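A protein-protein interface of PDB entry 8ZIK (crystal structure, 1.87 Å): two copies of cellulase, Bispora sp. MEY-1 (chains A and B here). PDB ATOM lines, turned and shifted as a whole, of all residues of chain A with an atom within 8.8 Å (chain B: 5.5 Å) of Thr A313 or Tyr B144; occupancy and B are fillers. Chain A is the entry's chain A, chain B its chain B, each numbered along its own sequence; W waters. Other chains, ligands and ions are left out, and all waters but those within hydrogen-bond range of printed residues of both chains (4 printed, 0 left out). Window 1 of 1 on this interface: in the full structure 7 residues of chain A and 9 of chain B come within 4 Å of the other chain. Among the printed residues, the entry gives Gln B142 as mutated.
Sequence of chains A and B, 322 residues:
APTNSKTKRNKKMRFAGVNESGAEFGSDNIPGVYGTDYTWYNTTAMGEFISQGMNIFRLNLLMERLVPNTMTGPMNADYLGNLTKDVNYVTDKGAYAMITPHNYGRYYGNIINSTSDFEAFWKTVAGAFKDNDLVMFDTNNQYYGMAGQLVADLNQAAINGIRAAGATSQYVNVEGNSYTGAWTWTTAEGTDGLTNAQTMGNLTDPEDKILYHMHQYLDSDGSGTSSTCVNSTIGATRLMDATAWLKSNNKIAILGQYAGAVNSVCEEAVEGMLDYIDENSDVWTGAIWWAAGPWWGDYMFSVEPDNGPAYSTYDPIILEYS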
ATOM      1  N   GLY A 260       8.682  24.416 -17.575  1.00  0.00           N
ATOM      2  CA  GLY A 260       8.458  25.824 -17.808  1.00  0.00           C
ATOM      3  C   GLY A 260       8.356  26.066 -19.304  1.00  0.00           C
ATOM      4  O   GLY A 260       8.859  25.294 -20.110  1.00  0.00           O
ATOM      5  N   ALA A 261       7.664  27.137 -19.663  1.00  0.00           N
ATOM      6  CA  ALA A 261       7.544  27.475 -21.070  1.00  0.00           C
ATOM      7  C   ALA A 261       8.801  28.209 -21.525  1.00  0.00           C
ATOM      8  O   ALA A 261       9.647  28.593 -20.715  1.00  0.00           O
ATOM      9  CB  ALA A 261       6.299  28.327 -21.319  1.00  0.00           C
ATOM     10  N   VAL A 262       8.918  28.402 -22.836  1.00  0.00           N
ATOM     11  CA  VAL A 262      10.105  29.017 -23.420  1.00  0.00           C
ATOM     12  C   VAL A 262       9.974  30.526 -23.274  1.00  0.00           C
ATOM     13  O   VAL A 262       9.536  31.224 -24.195  1.00  0.00           O
ATOM     14  CB  VAL A 262      10.298  28.622 -24.894  1.00  0.00           C
ATOM     15  CG1 VAL A 262      11.556  29.265 -25.440  1.00  0.00           C
ATOM     16  CG2 VAL A 262      10.389  27.107 -25.036  1.00  0.00           C
ATOM     17  N   ASN A 263      10.303  31.027 -22.093  1.00  0.00           N
ATOM     18  CA  ASN A 263      10.394  32.462 -21.875  1.00  0.00           C
ATOM     19  C   ASN A 263      11.322  32.672 -20.694  1.00  0.00           C
ATOM     20  O   ASN A 263      11.594  31.745 -19.927  1.00  0.00           O
ATOM     21  CB  ASN A 263       9.012  33.099 -21.651  1.00  0.00           C
ATOM     22  CG  ASN A 263       8.298  32.544 -20.437  1.00  0.00           C
ATOM     23  OD1 ASN A 263       8.701  32.805 -19.296  1.00  0.00           O
ATOM     24  ND2 ASN A 263       7.197  31.804 -20.670  1.00  0.00           N
ATOM     25  N   SER A 264      11.830  33.898 -20.574  1.00  0.00           N
ATOM     26  CA  SER A 264      12.940  34.135 -19.659  1.00  0.00           C
ATOM     27  C   SER A 264      12.557  33.882 -18.204  1.00  0.00           C
ATOM     28  O   SER A 264      13.348  33.305 -17.451  1.00  0.00           O
ATOM     29  CB  SER A 264      13.479  35.554 -19.843  1.00  0.00           C
ATOM     30  OG  SER A 264      14.182  35.645 -21.071  1.00  0.00           O
ATOM     31  N   CYS A 266      10.199  31.884 -16.946  1.00  0.00           N
ATOM     32  CA  CYS A 266      10.125  30.432 -16.797  1.00  0.00           C
ATOM     33  C   CYS A 266      11.515  29.801 -16.777  1.00  0.00           C
ATOM     34  O   CYS A 266      11.824  28.985 -15.897  1.00  0.00           O
ATOM     35  CB  CYS A 266       9.271  29.841 -17.917  1.00  0.00           C
ATOM     36  SG  CYS A 266       7.485  30.105 -17.709  1.00  0.00           S
ATOM     37  N   GLU A 267      12.376  30.174 -17.732  1.00  0.00           N
ATOM     38  CA  GLU A 267      13.721  29.604 -17.803  1.00  0.00           C
ATOM     39  C   GLU A 267      14.478  29.803 -16.494  1.00  0.00           C
ATOM     40  O   GLU A 267      15.026  28.852 -15.919  1.00  0.00           O
ATOM     41  CB  GLU A 267      14.488  30.241 -18.966  1.00  0.00           C
ATOM     42  CG  GLU A 267      15.810  29.560 -19.330  1.00  0.00           C
ATOM     43  CD  GLU A 267      16.418  30.147 -20.583  1.00  0.00           C
ATOM     44  OE1 GLU A 267      15.821  31.122 -21.094  1.00  0.00           O
ATOM     45  OE2 GLU A 267      17.490  29.659 -21.038  1.00  0.00           O
ATOM     46  N   GLU A 268      14.525  31.053 -16.015  1.00  0.00           N
ATOM     47  CA  GLU A 268      15.134  31.341 -14.721  1.00  0.00           C
ATOM     48  C   GLU A 268      14.485  30.540 -13.599  1.00  0.00           C
ATOM     49  O   GLU A 268      15.182  30.024 -12.718  1.00  0.00           O
ATOM     50  CB  GLU A 268      15.033  32.833 -14.417  1.00  0.00           C
ATOM     51  CG  GLU A 268      15.943  33.257 -13.316  1.00  0.00           C
ATOM     52  CD  GLU A 268      15.958  34.765 -13.103  1.00  0.00           C
ATOM     53  OE1 GLU A 268      15.250  35.504 -13.831  1.00  0.00           O
ATOM     54  OE2 GLU A 268      16.682  35.205 -12.190  1.00  0.00           O
ATOM     55  N   VAL A 270      12.994  27.663 -13.799  1.00  0.00           N
ATOM     56  CA  VAL A 270      13.354  26.251 -13.925  1.00  0.00           C
ATOM     57  C   VAL A 270      14.768  26.015 -13.412  1.00  0.00           C
ATOM     58  O   VAL A 270      15.009  25.099 -12.616  1.00  0.00           O
ATOM     59  CB  VAL A 270      13.196  25.769 -15.378  1.00  0.00           C
ATOM     60  CG1 VAL A 270      13.789  24.374 -15.538  1.00  0.00           C
ATOM     61  CG2 VAL A 270      11.720  25.766 -15.796  1.00  0.00           C
ATOM     62  N   GLU A 271      15.726  26.852 -13.842  1.00  0.00           N
ATOM     63  CA  GLU A 271      17.095  26.692 -13.365  1.00  0.00           C
ATOM     64  C   GLU A 271      17.145  26.772 -11.846  1.00  0.00           C
ATOM     65  O   GLU A 271      17.829  25.975 -11.191  1.00  0.00           O
ATOM     66  CB  GLU A 271      18.012  27.756 -13.982  1.00  0.00           C
ATOM     67  CG  GLU A 271      18.268  27.566 -15.452  1.00  0.00           C
ATOM     68  CD  GLU A 271      18.972  28.752 -16.107  1.00  0.00           C
ATOM     69  OE1 GLU A 271      18.547  29.916 -15.921  1.00  0.00           O
ATOM     70  OE2 GLU A 271      19.940  28.505 -16.852  1.00  0.00           O
ATOM     71  N   TRP A 289      11.626  15.924 -16.810  1.00  0.00           N
ATOM     72  CA  TRP A 289      10.908  16.968 -17.528  1.00  0.00           C
ATOM     73  C   TRP A 289       9.630  16.435 -18.166  1.00  0.00           C
ATOM     74  O   TRP A 289       9.585  15.305 -18.665  1.00  0.00           O
ATOM     75  CB  TRP A 289      11.806  17.549 -18.614  1.00  0.00           C
ATOM     76  CG  TRP A 289      11.160  18.589 -19.467  1.00  0.00           C
ATOM     77  CD1 TRP A 289      10.402  18.384 -20.578  1.00  0.00           C
ATOM     78  CD2 TRP A 289      11.247  20.013 -19.298  1.00  0.00           C
ATOM     79  NE1 TRP A 289       9.990  19.582 -21.102  1.00  0.00           N
ATOM     80  CE2 TRP A 289      10.507  20.601 -20.340  1.00  0.00           C
ATOM     81  CE3 TRP A 289      11.891  20.842 -18.373  1.00  0.00           C
ATOM     82  CZ2 TRP A 289      10.376  21.974 -20.476  1.00  0.00           C
ATOM     83  CZ3 TRP A 289      11.766  22.211 -18.510  1.00  0.00           C
ATOM     84  CH2 TRP A 289      11.017  22.765 -19.554  1.00  0.00           C
ATOM     85  N   MET A 300       3.827  23.559 -25.809  1.00  0.00           N
ATOM     86  CA  MET A 300       4.725  24.510 -25.152  1.00  0.00           C
ATOM     87  C   MET A 300       5.879  23.850 -24.417  1.00  0.00           C
ATOM     88  O   MET A 300       6.894  24.509 -24.173  1.00  0.00           O
ATOM     89  CB  MET A 300       4.017  25.383 -24.117  1.00  0.00           C
ATOM     90  CG  MET A 300       2.949  24.715 -23.292  1.00  0.00           C
ATOM     91  SD  MET A 300       1.942  25.994 -22.515  1.00  0.00           S
ATOM     92  CE  MET A 300       3.277  26.725 -21.597  1.00  0.00           C
ATOM     93  N   SER A 302       7.226  20.611 -25.089  1.00  0.00           N
ATOM     94  CA  SER A 302       7.817  19.455 -25.743  1.00  0.00           C
ATOM     95  C   SER A 302       9.302  19.704 -25.954  1.00  0.00           C
ATOM     96  O   SER A 302       9.683  20.708 -26.565  1.00  0.00           O
ATOM     97  CB  SER A 302       7.146  19.150 -27.076  1.00  0.00           C
ATOM     98  OG  SER A 302       7.954  18.216 -27.786  1.00  0.00           O
ATOM     99  N   VAL A 303      10.131  18.810 -25.425  1.00  0.00           N
ATOM    100  CA  VAL A 303      11.556  18.795 -25.720  1.00  0.00           C
ATOM    101  C   VAL A 303      11.913  17.654 -26.672  1.00  0.00           C
ATOM    102  O   VAL A 303      13.068  17.215 -26.714  1.00  0.00           O
ATOM    103  CB  VAL A 303      12.402  18.725 -24.441  1.00  0.00           C
ATOM    104  CG1 VAL A 303      12.196  19.986 -23.605  1.00  0.00           C
ATOM    105  CG2 VAL A 303      12.072  17.489 -23.654  1.00  0.00           C
ATOM    106  N   GLY A 308      10.401  19.709 -30.956  1.00  0.00           N
ATOM    107  CA  GLY A 308       9.940  20.277 -29.712  1.00  0.00           C
ATOM    108  C   GLY A 308      10.372  21.725 -29.533  1.00  0.00           C
ATOM    109  O   GLY A 308      11.563  22.042 -29.524  1.00  0.00           O
ATOM    110  N   PRO A 309       9.407  22.633 -29.382  1.00  0.00           N
ATOM    111  CA  PRO A 309       9.769  24.057 -29.262  1.00  0.00           C
ATOM    112  C   PRO A 309      10.634  24.348 -28.054  1.00  0.00           C
ATOM    113  O   PRO A 309      11.400  25.321 -28.077  1.00  0.00           O
ATOM    114  CB  PRO A 309       8.407  24.759 -29.165  1.00  0.00           C
ATOM    115  CG  PRO A 309       7.423  23.754 -29.775  1.00  0.00           C
ATOM    116  CD  PRO A 309       7.949  22.423 -29.381  1.00  0.00           C
ATOM    117  N   ALA A 310      10.542  23.535 -27.000  1.00  0.00           N
ATOM    118  CA  ALA A 310      11.318  23.731 -25.782  1.00  0.00           C
ATOM    119  C   ALA A 310      12.679  23.035 -25.802  1.00  0.00           C
ATOM    120  O   ALA A 310      13.432  23.146 -24.834  1.00  0.00           O
ATOM    121  CB  ALA A 310      10.516  23.245 -24.569  1.00  0.00           C
ATOM    122  N   TYR A 311      13.024  22.322 -26.867  1.00  0.00           N
ATOM    123  CA  TYR A 311      14.244  21.523 -26.842  1.00  0.00           C
ATOM    124  C   TYR A 311      15.496  22.394 -26.656  1.00  0.00           C
ATOM    125  O   TYR A 311      16.256  22.213 -25.697  1.00  0.00           O
ATOM    126  CB  TYR A 311      14.339  20.680 -28.119  1.00  0.00           C
ATOM    127  CG  TYR A 311      15.672  19.983 -28.248  1.00  0.00           C
ATOM    128  CD1 TYR A 311      15.931  18.806 -27.556  1.00  0.00           C
ATOM    129  CD2 TYR A 311      16.687  20.521 -29.033  1.00  0.00           C
ATOM    130  CE1 TYR A 311      17.153  18.174 -27.659  1.00  0.00           C
ATOM    131  CE2 TYR A 311      17.914  19.897 -29.136  1.00  0.00           C
ATOM    132  CZ  TYR A 311      18.140  18.728 -28.454  1.00  0.00           C
ATOM    133  OH  TYR A 311      19.357  18.112 -28.551  1.00  0.00           O
ATOM    134  N   SER A 312      15.725  23.355 -27.564  1.00  0.00           N
ATOM    135  CA  SER A 312      17.012  24.066 -27.563  1.00  0.00           C
ATOM    136  C   SER A 312      17.249  24.815 -26.257  1.00  0.00           C
ATOM    137  O   SER A 312      18.404  24.988 -25.846  1.00  0.00           O
ATOM    138  CB  SER A 312      17.102  25.048 -28.735  1.00  0.00           C
ATOM    139  OG  SER A 312      16.141  26.096 -28.617  1.00  0.00           O
ATOM    140  N   THR A 313      16.173  25.261 -25.597  1.00  0.00           N
ATOM    141  CA  THR A 313      16.276  25.977 -24.326  1.00  0.00           C
ATOM    142  C   THR A 313      16.481  25.027 -23.153  1.00  0.00           C
ATOM    143  O   THR A 313      17.371  25.236 -22.322  1.00  0.00           O
ATOM    144  CB  THR A 313      15.017  26.820 -24.087  1.00  0.00           C
ATOM    145  OG1 THR A 313      14.935  27.863 -25.065  1.00  0.00           O
ATOM    146  CG2 THR A 313      15.023  27.439 -22.687  1.00  0.00           C
ATOM    147  N   TYR A 314      15.664  23.977 -23.056  1.00  0.00           N
ATOM    148  CA  TYR A 314      15.644  23.187 -21.835  1.00  0.00           C
ATOM    149  C   TYR A 314      16.447  21.894 -21.903  1.00  0.00           C
ATOM    150  O   TYR A 314      16.812  21.362 -20.843  1.00  0.00           O
ATOM    151  CB  TYR A 314      14.195  22.899 -21.444  1.00  0.00           C
ATOM    152  CG  TYR A 314      13.519  24.130 -20.892  1.00  0.00           C
ATOM    153  CD1 TYR A 314      13.823  24.605 -19.626  1.00  0.00           C
ATOM    154  CD2 TYR A 314      12.605  24.837 -21.651  1.00  0.00           C
ATOM    155  CE1 TYR A 314      13.200  25.742 -19.111  1.00  0.00           C
ATOM    156  CE2 TYR A 314      11.988  25.966 -21.158  1.00  0.00           C
ATOM    157  CZ  TYR A 314      12.288  26.418 -19.889  1.00  0.00           C
ATOM    158  OH  TYR A 314      11.658  27.545 -19.403  1.00  0.00           O
ATOM    159  N   ASP A 315      16.764  21.385 -23.099  1.00  0.00           N
ATOM    160  CA  ASP A 315      17.683  20.251 -23.179  1.00  0.00           C
ATOM    161  C   ASP A 315      18.998  20.518 -22.458  1.00  0.00           C
ATOM    162  O   ASP A 315      19.402  19.678 -21.635  1.00  0.00           O
ATOM    163  CB  ASP A 315      17.935  19.882 -24.647  1.00  0.00           C
ATOM    164  CG  ASP A 315      18.923  18.741 -24.792  1.00  0.00           C
ATOM    165  OD1 ASP A 315      18.497  17.574 -24.693  1.00  0.00           O
ATOM    166  OD2 ASP A 315      20.130  18.999 -24.995  1.00  0.00           O
ATOM    167  N   PRO A 316      19.707  21.637 -22.705  1.00  0.00           N
ATOM    168  CA  PRO A 316      20.938  21.924 -21.939  1.00  0.00           C
ATOM    169  C   PRO A 316      20.704  22.096 -20.446  1.00  0.00           C
ATOM    170  O   PRO A 316      21.565  21.735 -19.632  1.00  0.00           O
ATOM    171  CB  PRO A 316      21.455  23.239 -22.561  1.00  0.00           C
ATOM    172  CG  PRO A 316      20.666  23.432 -23.830  1.00  0.00           C
ATOM    173  CD  PRO A 316      19.376  22.698 -23.671  1.00  0.00           C
ATOM    174  N   ILE A 317      19.568  22.673 -20.062  1.00  0.00           N
ATOM    175  CA  ILE A 317      19.298  22.870 -18.644  1.00  0.00           C
ATOM    176  C   ILE A 317      19.150  21.527 -17.940  1.00  0.00           C
ATOM    177  O   ILE A 317      19.682  21.324 -16.841  1.00  0.00           O
ATOM    178  CB  ILE A 317      18.059  23.769 -18.469  1.00  0.00           C
ATOM    179  CG1 ILE A 317      18.467  25.243 -18.632  1.00  0.00           C
ATOM    180  CG2 ILE A 317      17.383  23.537 -17.099  1.00  0.00           C
ATOM    181  CD1 ILE A 317      17.325  26.169 -19.027  1.00  0.00           C
ATOM    182  N   ILE A 318      18.457  20.574 -18.570  1.00  0.00           N
ATOM    183  CA  ILE A 318      18.305  19.267 -17.941  1.00  0.00           C
ATOM    184  C   ILE A 318      19.670  18.632 -17.710  1.00  0.00           C
ATOM    185  O   ILE A 318      19.909  17.991 -16.679  1.00  0.00           O
ATOM    186  CB  ILE A 318      17.396  18.365 -18.794  1.00  0.00           C
ATOM    187  CG1 ILE A 318      15.955  18.888 -18.781  1.00  0.00           C
ATOM    188  CG2 ILE A 318      17.484  16.937 -18.304  1.00  0.00           C
ATOM    189  CD1 ILE A 318      15.120  18.413 -19.951  1.00  0.00           C
ATOM    190  N   LEU A 319      20.589  18.799 -18.659  1.00  0.00           N
ATOM    191  CA  LEU A 319      21.892  18.161 -18.549  1.00  0.00           C
ATOM    192  C   LEU A 319      22.801  18.841 -17.536  1.00  0.00           C
ATOM    193  O   LEU A 319      23.887  18.320 -17.270  1.00  0.00           O
ATOM    194  CB  LEU A 319      22.560  18.108 -19.926  1.00  0.00           C
ATOM    195  CG  LEU A 319      21.812  17.256 -20.956  1.00  0.00           C
ATOM    196  CD1 LEU A 319      22.230  17.621 -22.360  1.00  0.00           C
ATOM    197  CD2 LEU A 319      22.081  15.777 -20.709  1.00  0.00           C
ATOM    198  N   TYR B 104      23.676  35.704 -26.084  1.00  0.00           N
ATOM    199  CA  TYR B 104      22.606  34.773 -26.424  1.00  0.00           C
ATOM    200  C   TYR B 104      21.271  35.490 -26.627  1.00  0.00           C
ATOM    201  O   TYR B 104      20.210  34.934 -26.335  1.00  0.00           O
ATOM    202  CB  TYR B 104      22.455  33.696 -25.349  1.00  0.00           C
ATOM    203  CG  TYR B 104      23.739  33.004 -24.973  1.00  0.00           C
ATOM    204  CD1 TYR B 104      24.265  31.988 -25.768  1.00  0.00           C
ATOM    205  CD2 TYR B 104      24.422  33.351 -23.811  1.00  0.00           C
ATOM    206  CE1 TYR B 104      25.448  31.346 -25.423  1.00  0.00           C
ATOM    207  CE2 TYR B 104      25.606  32.724 -23.456  1.00  0.00           C
ATOM    208  CZ  TYR B 104      26.109  31.715 -24.268  1.00  0.00           C
ATOM    209  OH  TYR B 104      27.276  31.082 -23.917  1.00  0.00           O
ATOM    210  N   ARG B 106      20.080  38.011 -24.951  1.00  0.00           N
ATOM    211  CA  ARG B 106      19.462  38.392 -23.694  1.00  0.00           C
ATOM    212  C   ARG B 106      20.230  39.550 -23.081  1.00  0.00           C
ATOM    213  O   ARG B 106      21.444  39.665 -23.245  1.00  0.00           O
ATOM    214  CB  ARG B 106      19.413  37.221 -22.721  1.00  0.00           C
ATOM    215  CG  ARG B 106      18.405  36.126 -23.163  1.00  0.00           C
ATOM    216  CD  ARG B 106      18.918  34.734 -22.879  1.00  0.00           C
ATOM    217  NE  ARG B 106      17.836  33.754 -22.941  1.00  0.00           N
ATOM    218  CZ  ARG B 106      17.494  33.085 -24.038  1.00  0.00           C
ATOM    219  NH1 ARG B 106      18.137  33.262 -25.183  1.00  0.00           N
ATOM    220  NH2 ARG B 106      16.480  32.223 -23.985  1.00  0.00           N
ATOM    221  N   ILE B 111      15.304  37.851 -22.649  1.00  0.00           N
ATOM    222  CA  ILE B 111      15.356  37.881 -24.101  1.00  0.00           C
ATOM    223  C   ILE B 111      15.026  39.269 -24.613  1.00  0.00           C
ATOM    224  O   ILE B 111      14.085  39.924 -24.154  1.00  0.00           O
ATOM    225  CB  ILE B 111      14.396  36.819 -24.669  1.00  0.00           C
ATOM    226  CG1 ILE B 111      14.925  35.429 -24.339  1.00  0.00           C
ATOM    227  CG2 ILE B 111      14.116  37.025 -26.167  1.00  0.00           C
ATOM    228  CD1 ILE B 111      13.975  34.324 -24.762  1.00  0.00           C
ATOM    229  N   GLN B 142      25.179  33.573 -30.454  1.00  0.00           N
ATOM    230  CA  GLN B 142      24.337  32.392 -30.238  1.00  0.00           C
ATOM    231  C   GLN B 142      22.965  32.722 -29.633  1.00  0.00           C
ATOM    232  O   GLN B 142      22.591  32.229 -28.566  1.00  0.00           O
ATOM    233  CB  GLN B 142      25.065  31.352 -29.376  1.00  0.00           C
ATOM    234  CG  GLN B 142      26.278  30.673 -30.046  1.00  0.00           C
ATOM    235  CD  GLN B 142      26.780  29.466 -29.259  1.00  0.00           C
ATOM    236  OE1 GLN B 142      26.423  29.280 -28.091  1.00  0.00           O
ATOM    237  NE2 GLN B 142      27.655  28.658 -29.885  1.00  0.00           N
ATOM    238  N   TYR B 143      22.167  33.485 -30.376  1.00  0.00           N
ATOM    239  CA  TYR B 143      20.749  33.535 -30.047  1.00  0.00           C
ATOM    240  C   TYR B 143      20.217  32.111 -29.896  1.00  0.00           C
ATOM    241  O   TYR B 143      20.631  31.199 -30.616  1.00  0.00           O
ATOM    242  CB  TYR B 143      19.942  34.248 -31.136  1.00  0.00           C
ATOM    243  CG  TYR B 143      20.426  35.630 -31.511  1.00  0.00           C
ATOM    244  CD1 TYR B 143      21.461  35.802 -32.420  1.00  0.00           C
ATOM    245  CD2 TYR B 143      19.817  36.766 -30.982  1.00  0.00           C
ATOM    246  CE1 TYR B 143      21.897  37.073 -32.781  1.00  0.00           C
ATOM    247  CE2 TYR B 143      20.249  38.042 -31.335  1.00  0.00           C
ATOM    248  CZ  TYR B 143      21.282  38.188 -32.245  1.00  0.00           C
ATOM    249  OH  TYR B 143      21.717  39.455 -32.599  1.00  0.00           O
ATOM    250  N   TYR B 144      19.290  31.920 -28.957  1.00  0.00           N
ATOM    251  CA  TYR B 144      18.638  30.616 -28.849  1.00  0.00           C
ATOM    252  C   TYR B 144      17.290  30.783 -28.177  1.00  0.00           C
ATOM    253  O   TYR B 144      17.041  31.770 -27.475  1.00  0.00           O
ATOM    254  CB  TYR B 144      19.501  29.613 -28.072  1.00  0.00           C
ATOM    255  CG  TYR B 144      19.460  29.824 -26.575  1.00  0.00           C
ATOM    256  CD1 TYR B 144      20.327  30.719 -25.959  1.00  0.00           C
ATOM    257  CD2 TYR B 144      18.530  29.165 -25.781  1.00  0.00           C
ATOM    258  CE1 TYR B 144      20.288  30.940 -24.594  1.00  0.00           C
ATOM    259  CE2 TYR B 144      18.475  29.380 -24.413  1.00  0.00           C
ATOM    260  CZ  TYR B 144      19.351  30.269 -23.823  1.00  0.00           C
ATOM    261  OH  TYR B 144      19.310  30.474 -22.461  1.00  0.00           O
ATOM    262  N   GLY B 145      16.424  29.795 -28.390  1.00  0.00           N
ATOM    263  CA  GLY B 145      15.168  29.763 -27.659  1.00  0.00           C
ATOM    264  C   GLY B 145      14.263  30.939 -27.921  1.00  0.00           C
ATOM    265  O   GLY B 145      13.523  31.350 -27.031  1.00  0.00           O
ATOM    266  N   MET B 146      14.293  31.481 -29.128  1.00  0.00           N
ATOM    267  CA  MET B 146      13.593  32.702 -29.482  1.00  0.00           C
ATOM    268  C   MET B 146      12.766  32.456 -30.730  1.00  0.00           C
ATOM    269  O   MET B 146      12.827  31.381 -31.329  1.00  0.00           O
ATOM    270  CB  MET B 146      14.602  33.837 -29.691  1.00  0.00           C
ATOM    271  CG  MET B 146      15.453  34.056 -28.467  1.00  0.00           C
ATOM    272  SD  MET B 146      16.816  35.236 -28.666  1.00  0.00           S
ATOM    273  CE  MET B 146      15.956  36.560 -29.494  1.00  0.00           C
ATOM    274  N   GLY B 176      22.449  33.342 -36.331  1.00  0.00           N
ATOM    275  CA  GLY B 176      21.107  32.816 -36.298  1.00  0.00           C
ATOM    276  C   GLY B 176      20.646  32.408 -34.908  1.00  0.00           C
ATOM    277  O   GLY B 176      21.380  32.466 -33.916  1.00  0.00           O
ATOM    278  N   ASN B 177      19.381  32.000 -34.868  1.00  0.00           N
ATOM    279  CA  ASN B 177      18.745  31.356 -33.730  1.00  0.00           C
ATOM    280  C   ASN B 177      19.402  29.989 -33.497  1.00  0.00           C
ATOM    281  O   ASN B 177      20.313  29.580 -34.222  1.00  0.00           O
ATOM    282  CB  ASN B 177      17.248  31.236 -34.020  1.00  0.00           C
ATOM    283  CG  ASN B 177      16.373  31.134 -32.762  1.00  0.00           C
ATOM    284  OD1 ASN B 177      16.834  31.290 -31.639  1.00  0.00           O
ATOM    285  ND2 ASN B 177      15.097  30.834 -32.973  1.00  0.00           N
ATOM    286  N   SER B 178      18.939  29.270 -32.473  1.00  0.00           N
ATOM    287  CA  SER B 178      19.401  27.907 -32.186  1.00  0.00           C
ATOM    288  C   SER B 178      20.933  27.808 -32.164  1.00  0.00           C
ATOM    289  O   SER B 178      21.538  26.875 -32.712  1.00  0.00           O
ATOM    290  CB  SER B 178      18.799  26.908 -33.188  1.00  0.00           C
ATOM    291  OG  SER B 178      17.370  27.014 -33.231  1.00  0.00           O
ATOM    292  N   TYR B 179      21.564  28.772 -31.495  1.00  0.00           N
ATOM    293  CA  TYR B 179      23.017  28.792 -31.319  1.00  0.00           C
ATOM    294  C   TYR B 179      23.751  28.925 -32.650  1.00  0.00           C
ATOM    295  O   TYR B 179      24.902  28.489 -32.780  1.00  0.00           O
ATOM    296  CB  TYR B 179      23.500  27.557 -30.554  1.00  0.00           C
ATOM    297  CG  TYR B 179      22.723  27.285 -29.277  1.00  0.00           C
ATOM    298  CD1 TYR B 179      21.639  26.405 -29.270  1.00  0.00           C
ATOM    299  CD2 TYR B 179      23.072  27.899 -28.083  1.00  0.00           C
ATOM    300  CE1 TYR B 179      20.934  26.153 -28.106  1.00  0.00           C
ATOM    301  CE2 TYR B 179      22.372  27.666 -26.919  1.00  0.00           C
ATOM    302  CZ  TYR B 179      21.300  26.785 -26.932  1.00  0.00           C
ATOM    303  OH  TYR B 179      20.598  26.543 -25.762  1.00  0.00           O
HETATM  304  O   HOH W   1      18.942  27.367 -21.559  1.00  0.00           O
HETATM  305  O   HOH W   2      14.432  30.493 -24.557  1.00  0.00           O
HETATM  306  O   HOH W   3      16.184  33.594 -20.591  1.00  0.00           O
HETATM  307  O   HOH W   4      16.493  28.040 -30.752  1.00  0.00           O
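No position is printed for both chains.
Of the 9 pairs that touch across the chains among the printed residues, none has its exchanged pair printed and touching as well.
The backbone carbonyl oxygen (O) of Ser A312 lies within hydrogen-bond range of the side-chain hydroxyl (OH) of Tyr B179 (2.7 Å).
The side-chain carboxylate (OE2) of Glu A267 lies within hydrogen-bond range of the side-chain hydroxyl (OH) of Tyr B144 (2.4 Å).
The guanidinium group (NH2) of Arg B106 is in salt-bridge range of the side-chain carboxylate (OE1) of Glu A267 (3.2 Å).
OG of Ser A264 lies within hydrogen-bond range of N of Ile B111, 2.9 Å away.
Among the printed residues, pairs that only touch across the chains: Val A262 with Gly B145, Ser A312 with Gly B145, Thr A313 with Tyr B144, Thr A313 with Gly B145 and Pro A316 with Tyr B179.
Hydrophobic or aromatic side chains of chain B within 4 Å of the printed part of chain A: Ile B111, Tyr B144 and Tyr B179.
Hydrophobic or aromatic side chains of chain A that line the printed part of chain B: Val A262 and Pro A316.
Water W3 lies within hydrogen-bond range of the side-chain carboxylate of Glu A267 (2.5 Å), the guanidinium group of Arg B106 (2.9 Å) and the side-chain hydroxyl of Ser A264 (2.9 Å).
Water W2 lies within hydrogen-bond range of the side-chain hydroxyl (OG1) of Thr A313, the guanidinium group (NH2) of Arg B106 and the backbone carbonyl oxygen (O) of Gly B145.
Water W1 lies within hydrogen-bond range of the backbone carbonyl oxygen of Thr A313, the side-chain carboxylate of Glu A267 and the side-chain hydroxyl of Tyr B144.
Water W4 lies within hydrogen-bond range of the side-chain hydroxyl (OG) of Ser B178 (2.8 Å), the side-chain hydroxyl (OG) of Ser A312 (2.9 Å), the backbone NH (N) of Gly B145 (2.9 Å) and the side-chain amide oxygen (OD1) of Asn B177 (3.4 Å).
The side-chain hydroxyl (OH) of Tyr A314 sits at hydrogen-bond distance from the backbone NH (N) of Glu A267 (3.2 Å).
O of Tyr B143 lies within hydrogen-bond range of N of Tyr B179 (2.7 Å).
The guanidinium group (NH1) of Arg B106 sits at hydrogen-bond distance from the backbone carbonyl oxygen (O) of Tyr B144 (2.9 Å).
NH1 of Arg B106 is in hydrogen-bond range of O of Tyr B104 (2.9 Å).
Printed residues of chain B within 4 Å of Val A262: Gly B145.
Thr A313 touches just these residues of chain B: Tyr B144 (3.9 Å) and Gly B145 (3.2 Å).
Of the printed residues of chain A, Arg B106 touches Glu A267.
The nearest residue of chain A that does not touch Tyr B144 is Ser A312 (4.2 Å).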
